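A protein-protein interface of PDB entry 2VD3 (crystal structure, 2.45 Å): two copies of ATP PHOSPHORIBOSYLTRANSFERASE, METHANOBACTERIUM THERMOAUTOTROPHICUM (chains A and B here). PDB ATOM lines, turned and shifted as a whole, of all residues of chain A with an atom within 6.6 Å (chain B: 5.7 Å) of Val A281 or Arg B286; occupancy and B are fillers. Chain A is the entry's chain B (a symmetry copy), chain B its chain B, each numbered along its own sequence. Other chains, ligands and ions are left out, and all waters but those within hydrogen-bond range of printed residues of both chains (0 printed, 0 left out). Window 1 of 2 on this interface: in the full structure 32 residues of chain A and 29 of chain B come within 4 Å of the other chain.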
ATOM      1  N   ARG A 217     -10.052  24.197   5.922  1.00  0.00           N
ATOM      2  CA  ARG A 217      -9.724  22.922   5.301  1.00  0.00           C
ATOM      3  C   ARG A 217     -10.935  22.016   5.216  1.00  0.00           C
ATOM      4  O   ARG A 217     -11.877  22.143   6.001  1.00  0.00           O
ATOM      5  CB  ARG A 217      -8.626  22.207   6.093  1.00  0.00           C
ATOM      6  CG  ARG A 217      -7.262  22.868   6.048  1.00  0.00           C
ATOM      7  CD  ARG A 217      -6.680  22.871   4.652  1.00  0.00           C
ATOM      8  NE  ARG A 217      -5.286  23.287   4.675  1.00  0.00           N
ATOM      9  CZ  ARG A 217      -4.868  24.540   4.529  1.00  0.00           C
ATOM     10  NH1 ARG A 217      -3.567  24.804   4.581  1.00  0.00           N
ATOM     11  NH2 ARG A 217      -5.743  25.528   4.337  1.00  0.00           N
ATOM     12  N   LEU A 218     -10.905  21.100   4.257  1.00  0.00           N
ATOM     13  CA  LEU A 218     -11.872  20.014   4.206  1.00  0.00           C
ATOM     14  C   LEU A 218     -11.275  18.820   4.948  1.00  0.00           C
ATOM     15  O   LEU A 218     -10.246  18.282   4.539  1.00  0.00           O
ATOM     16  CB  LEU A 218     -12.198  19.658   2.751  1.00  0.00           C
ATOM     17  CG  LEU A 218     -13.534  18.951   2.493  1.00  0.00           C
ATOM     18  CD1 LEU A 218     -14.720  19.898   2.664  1.00  0.00           C
ATOM     19  CD2 LEU A 218     -13.544  18.333   1.110  1.00  0.00           C
ATOM     20  N   VAL A 219     -11.885  18.438   6.064  1.00  0.00           N
ATOM     21  CA  VAL A 219     -11.432  17.255   6.793  1.00  0.00           C
ATOM     22  C   VAL A 219     -12.306  16.072   6.414  1.00  0.00           C
ATOM     23  O   VAL A 219     -13.520  16.199   6.349  1.00  0.00           O
ATOM     24  CB  VAL A 219     -11.382  17.473   8.343  1.00  0.00           C
ATOM     25  CG1 VAL A 219     -11.193  16.162   9.089  1.00  0.00           C
ATOM     26  CG2 VAL A 219     -10.265  18.406   8.689  1.00  0.00           C
ATOM     27  N   MET A 220     -11.668  14.933   6.158  1.00  0.00           N
ATOM     28  CA  MET A 220     -12.344  13.712   5.736  1.00  0.00           C
ATOM     29  C   MET A 220     -11.888  12.555   6.605  1.00  0.00           C
ATOM     30  O   MET A 220     -10.714  12.471   6.947  1.00  0.00           O
ATOM     31  CB  MET A 220     -11.998  13.389   4.281  1.00  0.00           C
ATOM     32  CG  MET A 220     -12.238  14.508   3.304  1.00  0.00           C
ATOM     33  SD  MET A 220     -11.696  14.059   1.647  1.00  0.00           S
ATOM     34  CE  MET A 220     -13.185  13.356   0.970  1.00  0.00           C
ATOM     35  N   GLU A 261      -8.344  25.670  10.600  1.00  0.00           N
ATOM     36  CA  GLU A 261      -7.035  25.266  11.133  1.00  0.00           C
ATOM     37  C   GLU A 261      -6.978  25.277  12.659  1.00  0.00           C
ATOM     38  O   GLU A 261      -6.376  24.385  13.273  1.00  0.00           O
ATOM     39  CB  GLU A 261      -5.923  26.182  10.621  1.00  0.00           C
ATOM     40  CG  GLU A 261      -5.762  26.216   9.127  1.00  0.00           C
ATOM     41  CD  GLU A 261      -4.929  25.081   8.562  1.00  0.00           C
ATOM     42  OE1 GLU A 261      -4.444  25.268   7.420  1.00  0.00           O
ATOM     43  OE2 GLU A 261      -4.762  24.027   9.239  1.00  0.00           O
ATOM     44  N   VAL A 264      -8.396  22.090  14.103  1.00  0.00           N
ATOM     45  CA  VAL A 264      -8.027  20.764  13.572  1.00  0.00           C
ATOM     46  C   VAL A 264      -7.333  19.806  14.562  1.00  0.00           C
ATOM     47  O   VAL A 264      -7.630  18.608  14.567  1.00  0.00           O
ATOM     48  CB  VAL A 264      -7.278  20.803  12.192  1.00  0.00           C
ATOM     49  CG1 VAL A 264      -7.881  21.832  11.289  1.00  0.00           C
ATOM     50  CG2 VAL A 264      -5.793  21.037  12.356  1.00  0.00           C
ATOM     51  N   PHE A 265      -6.430  20.329  15.388  1.00  0.00           N
ATOM     52  CA  PHE A 265      -5.706  19.484  16.333  1.00  0.00           C
ATOM     53  C   PHE A 265      -6.629  18.851  17.382  1.00  0.00           C
ATOM     54  O   PHE A 265      -6.642  17.619  17.536  1.00  0.00           O
ATOM     55  CB  PHE A 265      -4.559  20.246  17.007  1.00  0.00           C
ATOM     56  CG  PHE A 265      -3.784  19.416  17.985  1.00  0.00           C
ATOM     57  CD1 PHE A 265      -3.069  18.303  17.556  1.00  0.00           C
ATOM     58  CD2 PHE A 265      -3.780  19.739  19.337  1.00  0.00           C
ATOM     59  CE1 PHE A 265      -2.355  17.522  18.461  1.00  0.00           C
ATOM     60  CE2 PHE A 265      -3.068  18.975  20.248  1.00  0.00           C
ATOM     61  CZ  PHE A 265      -2.354  17.857  19.813  1.00  0.00           C
ATOM     62  N   ILE A 268      -9.005  16.373  15.628  1.00  0.00           N
ATOM     63  CA  ILE A 268      -8.338  15.099  15.342  1.00  0.00           C
ATOM     64  C   ILE A 268      -8.345  14.201  16.585  1.00  0.00           C
ATOM     65  O   ILE A 268      -8.750  13.040  16.506  1.00  0.00           O
ATOM     66  CB  ILE A 268      -6.902  15.299  14.757  1.00  0.00           C
ATOM     67  CG1 ILE A 268      -6.992  15.758  13.296  1.00  0.00           C
ATOM     68  CG2 ILE A 268      -6.078  14.008  14.831  1.00  0.00           C
ATOM     69  CD1 ILE A 268      -5.691  16.327  12.724  1.00  0.00           C
ATOM     70  N   ILE A 279      -7.754   9.955   8.475  1.00  0.00           N
ATOM     71  CA  ILE A 279      -8.162  11.356   8.493  1.00  0.00           C
ATOM     72  C   ILE A 279      -7.374  12.155   7.465  1.00  0.00           C
ATOM     73  O   ILE A 279      -6.142  12.164   7.474  1.00  0.00           O
ATOM     74  CB  ILE A 279      -8.002  11.992   9.899  1.00  0.00           C
ATOM     75  CG1 ILE A 279      -8.811  11.212  10.942  1.00  0.00           C
ATOM     76  CG2 ILE A 279      -8.397  13.480   9.877  1.00  0.00           C
ATOM     77  CD1 ILE A 279      -8.467  11.548  12.386  1.00  0.00           C
ATOM     78  N   LEU A 280      -8.093  12.832   6.579  1.00  0.00           N
ATOM     79  CA  LEU A 280      -7.451  13.567   5.502  1.00  0.00           C
ATOM     80  C   LEU A 280      -7.717  15.044   5.639  1.00  0.00           C
ATOM     81  O   LEU A 280      -8.813  15.459   6.035  1.00  0.00           O
ATOM     82  CB  LEU A 280      -7.948  13.091   4.135  1.00  0.00           C
ATOM     83  CG  LEU A 280      -8.033  11.583   3.863  1.00  0.00           C
ATOM     84  CD1 LEU A 280      -8.615  11.357   2.487  1.00  0.00           C
ATOM     85  CD2 LEU A 280      -6.670  10.891   4.017  1.00  0.00           C
ATOM     86  N   VAL A 281      -6.693  15.833   5.321  1.00  0.00           N
ATOM     87  CA  VAL A 281      -6.832  17.275   5.233  1.00  0.00           C
ATOM     88  C   VAL A 281      -6.561  17.653   3.785  1.00  0.00           C
ATOM     89  O   VAL A 281      -5.486  17.380   3.252  1.00  0.00           O
ATOM     90  CB  VAL A 281      -5.878  18.002   6.203  1.00  0.00           C
ATOM     91  CG1 VAL A 281      -5.993  19.500   6.036  1.00  0.00           C
ATOM     92  CG2 VAL A 281      -6.171  17.588   7.669  1.00  0.00           C
ATOM     93  N   VAL A 282      -7.565  18.251   3.155  1.00  0.00           N
ATOM     94  CA  VAL A 282      -7.553  18.565   1.733  1.00  0.00           C
ATOM     95  C   VAL A 282      -7.763  20.070   1.602  1.00  0.00           C
ATOM     96  O   VAL A 282      -8.623  20.629   2.287  1.00  0.00           O
ATOM     97  CB  VAL A 282      -8.673  17.772   0.989  1.00  0.00           C
ATOM     98  CG1 VAL A 282      -8.800  18.192  -0.481  1.00  0.00           C
ATOM     99  CG2 VAL A 282      -8.432  16.270   1.092  1.00  0.00           C
ATOM    100  N   PRO A 283      -6.975  20.733   0.732  1.00  0.00           N
ATOM    101  CA  PRO A 283      -7.030  22.191   0.632  1.00  0.00           C
ATOM    102  C   PRO A 283      -8.309  22.692  -0.019  1.00  0.00           C
ATOM    103  O   PRO A 283      -8.879  22.020  -0.885  1.00  0.00           O
ATOM    104  CB  PRO A 283      -5.827  22.525  -0.276  1.00  0.00           C
ATOM    105  CG  PRO A 283      -5.686  21.350  -1.135  1.00  0.00           C
ATOM    106  CD  PRO A 283      -5.997  20.171  -0.219  1.00  0.00           C
ATOM    107  N   GLU B  24       3.671  25.783   6.058  1.00  0.00           N
ATOM    108  CA  GLU B  24       2.465  26.276   5.393  1.00  0.00           C
ATOM    109  C   GLU B  24       1.455  25.138   5.277  1.00  0.00           C
ATOM    110  O   GLU B  24       0.312  25.273   5.706  1.00  0.00           O
ATOM    111  CB  GLU B  24       2.801  26.870   4.019  1.00  0.00           C
ATOM    112  CG  GLU B  24       1.589  27.118   3.089  1.00  0.00           C
ATOM    113  CD  GLU B  24       0.739  28.312   3.496  1.00  0.00           C
ATOM    114  OE1 GLU B  24       1.119  29.026   4.443  1.00  0.00           O
ATOM    115  OE2 GLU B  24      -0.319  28.547   2.865  1.00  0.00           O
ATOM    116  N   ASN B  25       1.907  24.014   4.730  1.00  0.00           N
ATOM    117  CA  ASN B  25       1.096  22.805   4.616  1.00  0.00           C
ATOM    118  C   ASN B  25       0.609  22.254   5.952  1.00  0.00           C
ATOM    119  O   ASN B  25      -0.364  21.502   5.995  1.00  0.00           O
ATOM    120  CB  ASN B  25       1.864  21.718   3.863  1.00  0.00           C
ATOM    121  CG  ASN B  25       2.143  22.095   2.435  1.00  0.00           C
ATOM    122  OD1 ASN B  25       1.395  22.850   1.826  1.00  0.00           O
ATOM    123  ND2 ASN B  25       3.235  21.571   1.889  1.00  0.00           N
ATOM    124  N   ALA B  26       1.292  22.616   7.031  1.00  0.00           N
ATOM    125  CA  ALA B  26       0.935  22.130   8.354  1.00  0.00           C
ATOM    126  C   ALA B  26      -0.029  23.076   9.079  1.00  0.00           C
ATOM    127  O   ALA B  26      -0.396  22.831  10.237  1.00  0.00           O
ATOM    128  CB  ALA B  26       2.197  21.878   9.191  1.00  0.00           C
ATOM    129  N   GLY B  27      -0.435  24.142   8.388  1.00  0.00           N
ATOM    130  CA  GLY B  27      -1.372  25.128   8.926  1.00  0.00           C
ATOM    131  C   GLY B  27      -0.712  26.198   9.777  1.00  0.00           C
ATOM    132  O   GLY B  27      -1.364  26.844  10.599  1.00  0.00           O
ATOM    133  N   THR B 205       2.096  17.171  15.087  1.00  0.00           N
ATOM    134  CA  THR B 205       1.025  16.462  14.403  1.00  0.00           C
ATOM    135  C   THR B 205       0.796  17.042  13.007  1.00  0.00           C
ATOM    136  O   THR B 205       0.719  16.299  12.028  1.00  0.00           O
ATOM    137  CB  THR B 205      -0.292  16.495  15.223  1.00  0.00           C
ATOM    138  OG1 THR B 205      -0.063  15.946  16.528  1.00  0.00           O
ATOM    139  CG2 THR B 205      -1.395  15.692  14.524  1.00  0.00           C
ATOM    140  N   GLY B 206       0.687  18.365  12.921  1.00  0.00           N
ATOM    141  CA  GLY B 206       0.543  19.034  11.632  1.00  0.00           C
ATOM    142  C   GLY B 206       1.672  18.637  10.701  1.00  0.00           C
ATOM    143  O   GLY B 206       1.441  18.167   9.574  1.00  0.00           O
ATOM    144  N   GLY B 209       1.616  14.999   9.740  1.00  0.00           N
ATOM    145  CA  GLY B 209       0.522  14.789   8.802  1.00  0.00           C
ATOM    146  C   GLY B 209       0.900  15.111   7.366  1.00  0.00           C
ATOM    147  O   GLY B 209       0.487  14.403   6.440  1.00  0.00           O
ATOM    148  N   VAL B 210       1.690  16.177   7.185  1.00  0.00           N
ATOM    149  CA  VAL B 210       2.196  16.573   5.863  1.00  0.00           C
ATOM    150  C   VAL B 210       3.100  15.498   5.256  1.00  0.00           C
ATOM    151  O   VAL B 210       2.922  15.104   4.094  1.00  0.00           O
ATOM    152  CB  VAL B 210       2.945  17.932   5.906  1.00  0.00           C
ATOM    153  CG1 VAL B 210       3.609  18.235   4.559  1.00  0.00           C
ATOM    154  CG2 VAL B 210       1.986  19.055   6.287  1.00  0.00           C
ATOM    155  N   ALA B 213       1.384  12.477   4.049  1.00  0.00           N
ATOM    156  CA  ALA B 213       0.561  12.706   2.858  1.00  0.00           C
ATOM    157  C   ALA B 213       1.374  12.626   1.559  1.00  0.00           C
ATOM    158  O   ALA B 213       0.813  12.403   0.486  1.00  0.00           O
ATOM    159  CB  ALA B 213      -0.169  14.038   2.956  1.00  0.00           C
ATOM    160  N   PRO B 283      -5.246  16.742  -4.564  1.00  0.00           N
ATOM    161  CA  PRO B 283      -4.164  16.691  -3.582  1.00  0.00           C
ATOM    162  C   PRO B 283      -4.664  16.482  -2.161  1.00  0.00           C
ATOM    163  O   PRO B 283      -5.760  16.929  -1.808  1.00  0.00           O
ATOM    164  CB  PRO B 283      -3.518  18.088  -3.698  1.00  0.00           C
ATOM    165  CG  PRO B 283      -4.619  18.960  -4.105  1.00  0.00           C
ATOM    166  CD  PRO B 283      -5.437  18.112  -5.074  1.00  0.00           C
ATOM    167  N   ILE B 284      -3.851  15.812  -1.358  1.00  0.00           N
ATOM    168  CA  ILE B 284      -4.082  15.707   0.066  1.00  0.00           C
ATOM    169  C   ILE B 284      -2.923  16.418   0.750  1.00  0.00           C
ATOM    170  O   ILE B 284      -1.763  16.128   0.475  1.00  0.00           O
ATOM    171  CB  ILE B 284      -4.173  14.234   0.525  1.00  0.00           C
ATOM    172  CG1 ILE B 284      -5.314  13.499  -0.199  1.00  0.00           C
ATOM    173  CG2 ILE B 284      -4.346  14.147   2.049  1.00  0.00           C
ATOM    174  CD1 ILE B 284      -5.315  11.959  -0.005  1.00  0.00           C
ATOM    175  N   GLU B 285      -3.243  17.367   1.620  1.00  0.00           N
ATOM    176  CA  GLU B 285      -2.240  18.139   2.342  1.00  0.00           C
ATOM    177  C   GLU B 285      -1.669  17.330   3.515  1.00  0.00           C
ATOM    178  O   GLU B 285      -0.445  17.266   3.706  1.00  0.00           O
ATOM    179  CB  GLU B 285      -2.888  19.417   2.860  1.00  0.00           C
ATOM    180  CG  GLU B 285      -1.943  20.570   3.057  1.00  0.00           C
ATOM    181  CD  GLU B 285      -2.595  21.730   3.764  1.00  0.00           C
ATOM    182  OE1 GLU B 285      -2.537  22.852   3.222  1.00  0.00           O
ATOM    183  OE2 GLU B 285      -3.172  21.525   4.857  1.00  0.00           O
ATOM    184  N   ARG B 286      -2.567  16.713   4.291  1.00  0.00           N
ATOM    185  CA  ARG B 286      -2.210  15.985   5.511  1.00  0.00           C
ATOM    186  C   ARG B 286      -2.998  14.693   5.638  1.00  0.00           C
ATOM    187  O   ARG B 286      -4.178  14.650   5.301  1.00  0.00           O
ATOM    188  CB  ARG B 286      -2.499  16.836   6.748  1.00  0.00           C
ATOM    189  CG  ARG B 286      -1.516  17.944   7.031  1.00  0.00           C
ATOM    190  CD  ARG B 286      -2.021  18.841   8.157  1.00  0.00           C
ATOM    191  NE  ARG B 286      -2.463  20.136   7.652  1.00  0.00           N
ATOM    192  CZ  ARG B 286      -3.062  21.079   8.372  1.00  0.00           C
ATOM    193  NH1 ARG B 286      -3.330  20.894   9.658  1.00  0.00           N
ATOM    194  NH2 ARG B 286      -3.404  22.220   7.791  1.00  0.00           N
ATOM    195  N   ILE B 287      -2.344  13.645   6.124  1.00  0.00           N
ATOM    196  CA  ILE B 287      -3.030  12.416   6.514  1.00  0.00           C
ATOM    197  C   ILE B 287      -2.694  12.039   7.953  1.00  0.00           C
ATOM    198  O   ILE B 287      -1.529  12.067   8.345  1.00  0.00           O
ATOM    199  CB  ILE B 287      -2.686  11.222   5.586  1.00  0.00           C
ATOM    200  CG1 ILE B 287      -2.969  11.587   4.131  1.00  0.00           C
ATOM    201  CG2 ILE B 287      -3.430   9.935   6.041  1.00  0.00           C
ATOM    202  CD1 ILE B 287      -2.721  10.482   3.158  1.00  0.00           C
ATOM    203  N   ILE B 288      -3.726  11.700   8.723  1.00  0.00           N
ATOM    204  CA  ILE B 288      -3.590  11.184  10.080  1.00  0.00           C
ATOM    205  C   ILE B 288      -4.386   9.886  10.139  1.00  0.00           C
ATOM    206  O   ILE B 288      -5.623   9.917  10.163  1.00  0.00           O
ATOM    207  CB  ILE B 288      -4.161  12.151  11.156  1.00  0.00           C
ATOM    208  CG1 ILE B 288      -3.819  13.626  10.863  1.00  0.00           C
ATOM    209  CG2 ILE B 288      -3.743  11.710  12.572  1.00  0.00           C
ATOM    210  CD1 ILE B 288      -2.384  14.041  11.141  1.00  0.00           C
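OE1 of Glu B285 is in salt-bridge range of NH1 of Arg A217 (2.6 Å). The backbone NH of Glu B285 is in hydrogen-bond range of the backbone carbonyl oxygen of Val A281 (2.8 Å). The side-chain carboxylate (OE2) of Glu A261 lies within salt-bridge range of the guanidinium group (NH2) of Arg B286, at 2.7 Å. N of Val A281 is in hydrogen-bond range of O of Arg B286. N of Ile A279 lies within hydrogen-bond range of O of Ile B288.
O of Asn B25 is in hydrogen-bond range of NE of Arg B286 (3.0 Å). O of Gly B209 sits at hydrogen-bond distance from N of Ile B287, 2.9 Å away. NH2 of Arg B286 lies within salt-bridge range of OE2 of Glu B285. NH1 of Arg A217 is in salt-bridge range of OE1 of Glu A261, 3.0 Å away. The backbone carbonyl oxygen of Leu A218 lies within hydrogen-bond range of the backbone NH of Val A282 (3.0 Å). O of Met A220 lies within hydrogen-bond range of N of Leu A280 (2.7 Å).
Pro B283 touches its own counterpart, Pro A283. 1 position is printed for both chains.
Among the printed residues, merely in contact across the chains: Arg A217 with Arg B286, Glu A261 with Gly B27, Val A264 with Arg B286, Phe A265 with Thr B205, Ile A268 with Ile B288, Ile A279 with Arg B286, Ile A279 with Ile B287, Leu A280 with Arg B286, Leu A280 with Ile B287, Val A281 with Ile B284, Val A282 with Pro B283 and Pro A283 with Pro B283.
Of the 13 printed residues of chain A, 10 touch a printed residue of chain B. Hydrophobic or aromatic side chains of chain A within 4 Å of the printed part of chain B: Val A264, Phe A265, Ile A268, Ile A279, Leu A280, Val A281, Val A282 and Pro A283. Of the 15 printed residues of chain B, 8 touch a printed residue of chain A. Hydrophobic or aromatic side chains of chain B within 4 Å of the printed part of chain A: Pro B283, Ile B284, Ile B287 and Ile B288.
Printed residues of chain B within 4 Å of Val A264: Arg B286 (3.7 Å). Printed residues of chain B within 4 Å of Phe A265: Thr B205. Of the printed residues of chain B, Ile A268 touches Ile B288. Val A281 touches just these residues of chain B: Ile B284, Glu B285 and Arg B286. Of the printed residues of chain B, Val A282 touches Pro B283 (3.5 Å). Ala B213 touches none of the printed residues of chain A. Of the printed residues of chain A, Pro B283 touches Val A282 and Pro A283. Of chain A, only Arg A217, Glu A261, Val A264, Ile A279, Leu A280 and Val A281 come within 4 Å of Arg B286. The nearest residue of chain B that does not touch Val A281 is Ile B287 (4.9 Å). The nearest residue of chain A that does not touch Arg B286 is Val A282 (5.4 Å).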
